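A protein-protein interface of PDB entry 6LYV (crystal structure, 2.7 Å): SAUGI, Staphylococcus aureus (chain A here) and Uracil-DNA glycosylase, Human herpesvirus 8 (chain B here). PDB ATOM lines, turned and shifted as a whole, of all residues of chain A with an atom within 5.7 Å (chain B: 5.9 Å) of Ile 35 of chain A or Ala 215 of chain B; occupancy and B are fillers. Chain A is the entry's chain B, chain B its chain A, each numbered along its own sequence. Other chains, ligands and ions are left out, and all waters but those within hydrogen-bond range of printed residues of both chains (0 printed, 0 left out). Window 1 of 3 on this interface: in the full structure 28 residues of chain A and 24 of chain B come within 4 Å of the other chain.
The guanidinium group of Arg 220 of chain B is in hydrogen-bond range of the backbone carbonyl oxygen of Ile 35 of chain A, 2.9 Å away. The guanidinium group (NH1) of Arg 220 of chain B lies within hydrogen-bond range of the side-chain sulfur (SD) of Met 89 of chain A, at 3.1 Å.
The side-chain amide oxygen (OE1) of Gln 209 of chain B lies close to the backbone carbonyl oxygen (O) of Ala 215 of chain B (2.7 Å). N of Ser 212 of chain B sits at hydrogen-bond distance from ND1 of His 210 of chain B (3.0 Å). The side-chain hydroxyl (OG) of Ser 212 of chain B sits close to the backbone NH (N) of Leu 214 of chain B. The backbone carbonyl oxygen (O) of Ala 215 of chain B sits at hydrogen-bond distance from the guanidinium group (NH2) of Arg 226 of chain B (2.5 Å). The backbone carbonyl oxygen of Leu 217 of chain B sits at hydrogen-bond distance from the guanidinium group of Arg 226 of chain B, at 2.9 Å. N of Leu 51 of chain A sits at hydrogen-bond distance from O of Glu 30 of chain A (2.7 Å).
Among the printed residues, merely in contact across the chains: Glu 30 of chain A with His 210 of chain B (3.7 Å), Asp 33 of chain A with Arg 220 of chain B (3.4 Å), Asp 34 of chain A with Leu 214 of chain B (3.6 Å), Asp 34 of chain A with Ala 215 of chain B (3.4 Å), Asp 34 of chain A with Arg 220 of chain B (3.5 Å), Ile 35 of chain A with Leu 214 of chain B (3.2 Å), Ile 35 of chain A with Ala 215 of chain B (3.7 Å), Leu 36 of chain A with Arg 220 of chain B (3.2 Å), Pro 37 of chain A with Arg 220 of chain B (3.3 Å), Thr 53 of chain A with Leu 214 of chain B (3.6 Å), Leu 71 of chain A with Leu 214 of chain B (3.8 Å) and Met 89 of chain A with Leu 217 of chain B (3.5 Å).
Of chain B, only Leu 214 (3.2 Å), Ala 215 (3.7 Å) and Arg 220 (2.9 Å) come within 4 Å of Ile 35 of chain A. Of the printed residues of chain B, Asp 34 of chain A touches Leu 214, Ala 215 and Arg 220. Of the printed residues of chain B, Leu 71 of chain A touches Leu 214 (3.8 Å). Printed residues of chain A within 4 Å of Leu 214 of chain B: Asp 34, Ile 35, Thr 53 and Leu 71. Printed residues of chain A within 4 Å of His 210 of chain B: Glu 30 (3.7 Å). Of the printed residues of chain B, Leu 36 of chain A touches Arg 220 (3.2 Å). Arg 226 of chain B touches none of the printed residues of chain A. Ser 212 of chain B touches none of the printed residues of chain A.
Of the 12 printed residues of chain A, 9 touch a printed residue of chain B. Hydrophobic or aromatic side chains of chain A that line the printed part of chain B: Ile 35, Pro 37, Leu 71 and Met 89.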
ATOM      1  N   GLU A  30      -1.273 -15.437  26.228  1.00  0.00           N
ATOM      2  CA  GLU A  30      -0.873 -16.256  25.092  1.00  0.00           C
ATOM      3  C   GLU A  30      -1.658 -15.802  23.866  1.00  0.00           C
ATOM      4  O   GLU A  30      -2.784 -15.313  23.988  1.00  0.00           O
ATOM      5  CB  GLU A  30      -1.105 -17.746  25.380  1.00  0.00           C
ATOM      6  CG  GLU A  30      -0.473 -18.689  24.370  1.00  0.00           C
ATOM      7  CD  GLU A  30       0.986 -18.379  24.133  1.00  0.00           C
ATOM      8  OE1 GLU A  30       1.736 -18.283  25.125  1.00  0.00           O
ATOM      9  OE2 GLU A  30       1.380 -18.206  22.961  1.00  0.00           O
ATOM     10  N   ILE A  31      -1.047 -15.952  22.687  1.00  0.00           N
ATOM     11  CA  ILE A  31      -1.731 -15.574  21.453  1.00  0.00           C
ATOM     12  C   ILE A  31      -2.925 -16.491  21.223  1.00  0.00           C
ATOM     13  O   ILE A  31      -2.902 -17.686  21.552  1.00  0.00           O
ATOM     14  CB  ILE A  31      -0.784 -15.600  20.239  1.00  0.00           C
ATOM     15  CG1 ILE A  31       0.211 -16.749  20.357  1.00  0.00           C
ATOM     16  CG2 ILE A  31      -0.073 -14.269  20.073  1.00  0.00           C
ATOM     17  CD1 ILE A  31       1.115 -16.868  19.168  1.00  0.00           C
ATOM     18  N   ALA A  32      -3.977 -15.929  20.627  1.00  0.00           N
ATOM     19  CA  ALA A  32      -5.188 -16.700  20.375  1.00  0.00           C
ATOM     20  C   ALA A  32      -4.941 -17.890  19.457  1.00  0.00           C
ATOM     21  O   ALA A  32      -5.693 -18.868  19.520  1.00  0.00           O
ATOM     22  CB  ALA A  32      -6.268 -15.793  19.780  1.00  0.00           C
ATOM     23  N   ASP A  33      -3.896 -17.839  18.623  1.00  0.00           N
ATOM     24  CA  ASP A  33      -3.642 -18.926  17.683  1.00  0.00           C
ATOM     25  C   ASP A  33      -3.401 -20.248  18.396  1.00  0.00           C
ATOM     26  O   ASP A  33      -3.735 -21.310  17.858  1.00  0.00           O
ATOM     27  CB  ASP A  33      -2.449 -18.588  16.790  1.00  0.00           C
ATOM     28  CG  ASP A  33      -2.564 -17.214  16.164  1.00  0.00           C
ATOM     29  OD1 ASP A  33      -3.566 -16.522  16.430  1.00  0.00           O
ATOM     30  OD2 ASP A  33      -1.658 -16.827  15.397  1.00  0.00           O
ATOM     31  N   ASP A  34      -2.817 -20.210  19.593  1.00  0.00           N
ATOM     32  CA  ASP A  34      -2.514 -21.424  20.340  1.00  0.00           C
ATOM     33  C   ASP A  34      -3.641 -21.870  21.261  1.00  0.00           C
ATOM     34  O   ASP A  34      -3.579 -22.989  21.780  1.00  0.00           O
ATOM     35  CB  ASP A  34      -1.241 -21.237  21.173  1.00  0.00           C
ATOM     36  CG  ASP A  34      -0.038 -20.867  20.332  1.00  0.00           C
ATOM     37  OD1 ASP A  34      -0.227 -20.477  19.161  1.00  0.00           O
ATOM     38  OD2 ASP A  34       1.098 -20.969  20.846  1.00  0.00           O
ATOM     39  N   ILE A  35      -4.660 -21.042  21.475  1.00  0.00           N
ATOM     40  CA  ILE A  35      -5.683 -21.294  22.486  1.00  0.00           C
ATOM     41  C   ILE A  35      -7.023 -21.664  21.856  1.00  0.00           C
ATOM     42  O   ILE A  35      -7.616 -22.690  22.193  1.00  0.00           O
ATOM     43  CB  ILE A  35      -5.833 -20.081  23.432  1.00  0.00           C
ATOM     44  CG1 ILE A  35      -4.471 -19.653  23.980  1.00  0.00           C
ATOM     45  CG2 ILE A  35      -6.766 -20.411  24.575  1.00  0.00           C
ATOM     46  CD1 ILE A  35      -3.789 -20.717  24.798  1.00  0.00           C
ATOM     47  N   LEU A  36      -7.502 -20.853  20.929  1.00  0.00           N
ATOM     48  CA  LEU A  36      -8.852 -20.962  20.397  1.00  0.00           C
ATOM     49  C   LEU A  36      -8.866 -21.746  19.093  1.00  0.00           C
ATOM     50  O   LEU A  36      -7.825 -21.929  18.457  1.00  0.00           O
ATOM     51  CB  LEU A  36      -9.432 -19.565  20.170  1.00  0.00           C
ATOM     52  CG  LEU A  36      -9.769 -18.810  21.447  1.00  0.00           C
ATOM     53  CD1 LEU A  36     -10.155 -17.386  21.106  1.00  0.00           C
ATOM     54  CD2 LEU A  36     -10.886 -19.527  22.185  1.00  0.00           C
ATOM     55  N   PRO A  37     -10.029 -22.259  18.682  1.00  0.00           N
ATOM     56  CA  PRO A  37     -10.100 -23.003  17.419  1.00  0.00           C
ATOM     57  C   PRO A  37      -9.579 -22.184  16.243  1.00  0.00           C
ATOM     58  O   PRO A  37      -9.698 -20.959  16.209  1.00  0.00           O
ATOM     59  CB  PRO A  37     -11.594 -23.310  17.275  1.00  0.00           C
ATOM     60  CG  PRO A  37     -12.087 -23.369  18.674  1.00  0.00           C
ATOM     61  CD  PRO A  37     -11.295 -22.339  19.433  1.00  0.00           C
ATOM     62  N   LEU A  51      -4.196 -12.988  24.202  1.00  0.00           N
ATOM     63  CA  LEU A  51      -5.336 -13.173  25.086  1.00  0.00           C
ATOM     64  C   LEU A  51      -4.857 -13.251  26.529  1.00  0.00           C
ATOM     65  O   LEU A  51      -3.870 -13.930  26.827  1.00  0.00           O
ATOM     66  CB  LEU A  51      -6.103 -14.450  24.737  1.00  0.00           C
ATOM     67  CG  LEU A  51      -6.700 -14.575  23.338  1.00  0.00           C
ATOM     68  CD1 LEU A  51      -7.476 -15.876  23.215  1.00  0.00           C
ATOM     69  CD2 LEU A  51      -7.582 -13.383  23.013  1.00  0.00           C
ATOM     70  N   THR A  53      -5.614 -14.946  29.741  1.00  0.00           N
ATOM     71  CA  THR A  53      -6.329 -16.170  30.071  1.00  0.00           C
ATOM     72  C   THR A  53      -6.333 -16.389  31.574  1.00  0.00           C
ATOM     73  O   THR A  53      -5.358 -16.070  32.260  1.00  0.00           O
ATOM     74  CB  THR A  53      -5.697 -17.379  29.393  1.00  0.00           C
ATOM     75  OG1 THR A  53      -4.512 -17.749  30.106  1.00  0.00           O
ATOM     76  CG2 THR A  53      -5.335 -17.044  27.951  1.00  0.00           C
ATOM     77  N   LEU A  71     -11.322 -16.269  28.925  1.00  0.00           N
ATOM     78  CA  LEU A  71     -10.371 -15.645  28.016  1.00  0.00           C
ATOM     79  C   LEU A  71     -10.819 -14.224  27.696  1.00  0.00           C
ATOM     80  O   LEU A  71     -11.960 -14.008  27.277  1.00  0.00           O
ATOM     81  CB  LEU A  71     -10.236 -16.458  26.725  1.00  0.00           C
ATOM     82  CG  LEU A  71     -10.017 -17.968  26.868  1.00  0.00           C
ATOM     83  CD1 LEU A  71      -9.858 -18.628  25.511  1.00  0.00           C
ATOM     84  CD2 LEU A  71      -8.812 -18.270  27.743  1.00  0.00           C
ATOM     85  N   MET A  89     -11.984 -28.420  24.346  1.00  0.00           N
ATOM     86  CA  MET A  89     -12.401 -27.102  24.819  1.00  0.00           C
ATOM     87  C   MET A  89     -13.903 -26.946  24.620  1.00  0.00           C
ATOM     88  O   MET A  89     -14.375 -26.809  23.487  1.00  0.00           O
ATOM     89  CB  MET A  89     -11.659 -25.992  24.083  1.00  0.00           C
ATOM     90  CG  MET A  89     -11.281 -24.820  24.976  1.00  0.00           C
ATOM     91  SD  MET A  89     -10.453 -23.503  24.073  1.00  0.00           S
ATOM     92  CE  MET A  89      -9.420 -22.814  25.359  1.00  0.00           C
ATOM     93  N   GLN B 209       5.277 -24.446  22.862  1.00  0.00           N
ATOM     94  CA  GLN B 209       4.084 -23.755  23.317  1.00  0.00           C
ATOM     95  C   GLN B 209       4.086 -23.632  24.838  1.00  0.00           C
ATOM     96  O   GLN B 209       4.836 -24.308  25.546  1.00  0.00           O
ATOM     97  CB  GLN B 209       2.832 -24.498  22.858  1.00  0.00           C
ATOM     98  CG  GLN B 209       2.752 -24.666  21.359  1.00  0.00           C
ATOM     99  CD  GLN B 209       1.649 -25.611  20.936  1.00  0.00           C
ATOM    100  OE1 GLN B 209       0.670 -25.804  21.652  1.00  0.00           O
ATOM    101  NE2 GLN B 209       1.820 -26.232  19.777  1.00  0.00           N
ATOM    102  N   HIS B 210       3.229 -22.755  25.335  1.00  0.00           N
ATOM    103  CA  HIS B 210       3.108 -22.587  26.772  1.00  0.00           C
ATOM    104  C   HIS B 210       2.583 -23.874  27.406  1.00  0.00           C
ATOM    105  O   HIS B 210       1.712 -24.540  26.834  1.00  0.00           O
ATOM    106  CB  HIS B 210       2.174 -21.420  27.091  1.00  0.00           C
ATOM    107  CG  HIS B 210       2.288 -20.924  28.498  1.00  0.00           C
ATOM    108  ND1 HIS B 210       1.636 -21.525  29.551  1.00  0.00           N
ATOM    109  CD2 HIS B 210       2.983 -19.889  29.025  1.00  0.00           C
ATOM    110  CE1 HIS B 210       1.920 -20.879  30.668  1.00  0.00           C
ATOM    111  NE2 HIS B 210       2.735 -19.882  30.376  1.00  0.00           N
ATOM    112  N   PRO B 211       3.093 -24.264  28.576  1.00  0.00           N
ATOM    113  CA  PRO B 211       2.628 -25.510  29.202  1.00  0.00           C
ATOM    114  C   PRO B 211       1.190 -25.454  29.692  1.00  0.00           C
ATOM    115  O   PRO B 211       0.670 -26.493  30.118  1.00  0.00           O
ATOM    116  CB  PRO B 211       3.600 -25.698  30.371  1.00  0.00           C
ATOM    117  CG  PRO B 211       4.077 -24.312  30.682  1.00  0.00           C
ATOM    118  CD  PRO B 211       4.154 -23.610  29.362  1.00  0.00           C
ATOM    119  N   SER B 212       0.541 -24.293  29.650  1.00  0.00           N
ATOM    120  CA  SER B 212      -0.829 -24.187  30.127  1.00  0.00           C
ATOM    121  C   SER B 212      -1.726 -25.175  29.389  1.00  0.00           C
ATOM    122  O   SER B 212      -1.545 -25.403  28.187  1.00  0.00           O
ATOM    123  CB  SER B 212      -1.370 -22.774  29.930  1.00  0.00           C
ATOM    124  OG  SER B 212      -2.751 -22.727  30.249  1.00  0.00           O
ATOM    125  N   PRO B 213      -2.695 -25.787  30.072  1.00  0.00           N
ATOM    126  CA  PRO B 213      -3.630 -26.682  29.374  1.00  0.00           C
ATOM    127  C   PRO B 213      -4.415 -25.988  28.276  1.00  0.00           C
ATOM    128  O   PRO B 213      -4.863 -26.658  27.339  1.00  0.00           O
ATOM    129  CB  PRO B 213      -4.555 -27.171  30.499  1.00  0.00           C
ATOM    130  CG  PRO B 213      -3.782 -26.961  31.755  1.00  0.00           C
ATOM    131  CD  PRO B 213      -2.943 -25.742  31.523  1.00  0.00           C
ATOM    132  N   LEU B 214      -4.592 -24.667  28.360  1.00  0.00           N
ATOM    133  CA  LEU B 214      -5.317 -23.926  27.335  1.00  0.00           C
ATOM    134  C   LEU B 214      -4.599 -23.927  25.993  1.00  0.00           C
ATOM    135  O   LEU B 214      -5.221 -23.620  24.970  1.00  0.00           O
ATOM    136  CB  LEU B 214      -5.547 -22.487  27.793  1.00  0.00           C
ATOM    137  CG  LEU B 214      -6.312 -22.311  29.106  1.00  0.00           C
ATOM    138  CD1 LEU B 214      -6.543 -20.840  29.367  1.00  0.00           C
ATOM    139  CD2 LEU B 214      -7.630 -23.065  29.077  1.00  0.00           C
ATOM    140  N   ALA B 215      -3.306 -24.242  25.976  1.00  0.00           N
ATOM    141  CA  ALA B 215      -2.533 -24.275  24.746  1.00  0.00           C
ATOM    142  C   ALA B 215      -2.222 -25.689  24.273  1.00  0.00           C
ATOM    143  O   ALA B 215      -1.540 -25.850  23.258  1.00  0.00           O
ATOM    144  CB  ALA B 215      -1.229 -23.490  24.927  1.00  0.00           C
ATOM    145  N   SER B 216      -2.716 -26.712  24.964  1.00  0.00           N
ATOM    146  CA  SER B 216      -2.397 -28.101  24.654  1.00  0.00           C
ATOM    147  C   SER B 216      -3.431 -28.779  23.761  1.00  0.00           C
ATOM    148  O   SER B 216      -3.266 -29.961  23.440  1.00  0.00           O
ATOM    149  CB  SER B 216      -2.240 -28.903  25.948  1.00  0.00           C
ATOM    150  OG  SER B 216      -3.452 -28.922  26.678  1.00  0.00           O
ATOM    151  N   LEU B 217      -4.488 -28.072  23.364  1.00  0.00           N
ATOM    152  CA  LEU B 217      -5.613 -28.649  22.644  1.00  0.00           C
ATOM    153  C   LEU B 217      -5.324 -28.751  21.150  1.00  0.00           C
ATOM    154  O   LEU B 217      -4.601 -27.936  20.578  1.00  0.00           O
ATOM    155  CB  LEU B 217      -6.841 -27.772  22.834  1.00  0.00           C
ATOM    156  CG  LEU B 217      -7.048 -27.306  24.269  1.00  0.00           C
ATOM    157  CD1 LEU B 217      -8.201 -26.342  24.322  1.00  0.00           C
ATOM    158  CD2 LEU B 217      -7.314 -28.491  25.164  1.00  0.00           C
ATOM    159  N   ARG B 220      -5.787 -26.196  16.741  1.00  0.00           N
ATOM    160  CA  ARG B 220      -5.312 -24.825  16.811  1.00  0.00           C
ATOM    161  C   ARG B 220      -4.312 -24.597  15.682  1.00  0.00           C
ATOM    162  O   ARG B 220      -4.112 -25.455  14.815  1.00  0.00           O
ATOM    163  CB  ARG B 220      -4.687 -24.536  18.180  1.00  0.00           C
ATOM    164  CG  ARG B 220      -5.680 -24.207  19.286  1.00  0.00           C
ATOM    165  CD  ARG B 220      -6.469 -25.437  19.711  1.00  0.00           C
ATOM    166  NE  ARG B 220      -7.503 -25.132  20.695  1.00  0.00           N
ATOM    167  CZ  ARG B 220      -8.810 -25.222  20.463  1.00  0.00           C
ATOM    168  NH1 ARG B 220      -9.675 -24.917  21.418  1.00  0.00           N
ATOM    169  NH2 ARG B 220      -9.251 -25.635  19.283  1.00  0.00           N
ATOM    170  N   ARG B 226       4.164 -28.721  20.404  1.00  0.00           N
ATOM    171  CA  ARG B 226       3.370 -28.956  21.601  1.00  0.00           C
ATOM    172  C   ARG B 226       4.285 -29.129  22.803  1.00  0.00           C
ATOM    173  O   ARG B 226       5.394 -29.658  22.697  1.00  0.00           O
ATOM    174  CB  ARG B 226       2.504 -30.206  21.434  1.00  0.00           C
ATOM    175  CG  ARG B 226       1.408 -30.050  20.413  1.00  0.00           C
ATOM    176  CD  ARG B 226       0.366 -29.079  20.921  1.00  0.00           C
ATOM    177  NE  ARG B 226      -0.706 -28.868  19.958  1.00  0.00           N
ATOM    178  CZ  ARG B 226      -1.759 -28.093  20.184  1.00  0.00           C
ATOM    179  NH1 ARG B 226      -2.693 -27.947  19.253  1.00  0.00           N
ATOM    180  NH2 ARG B 226      -1.888 -27.476  21.352  1.00  0.00           N
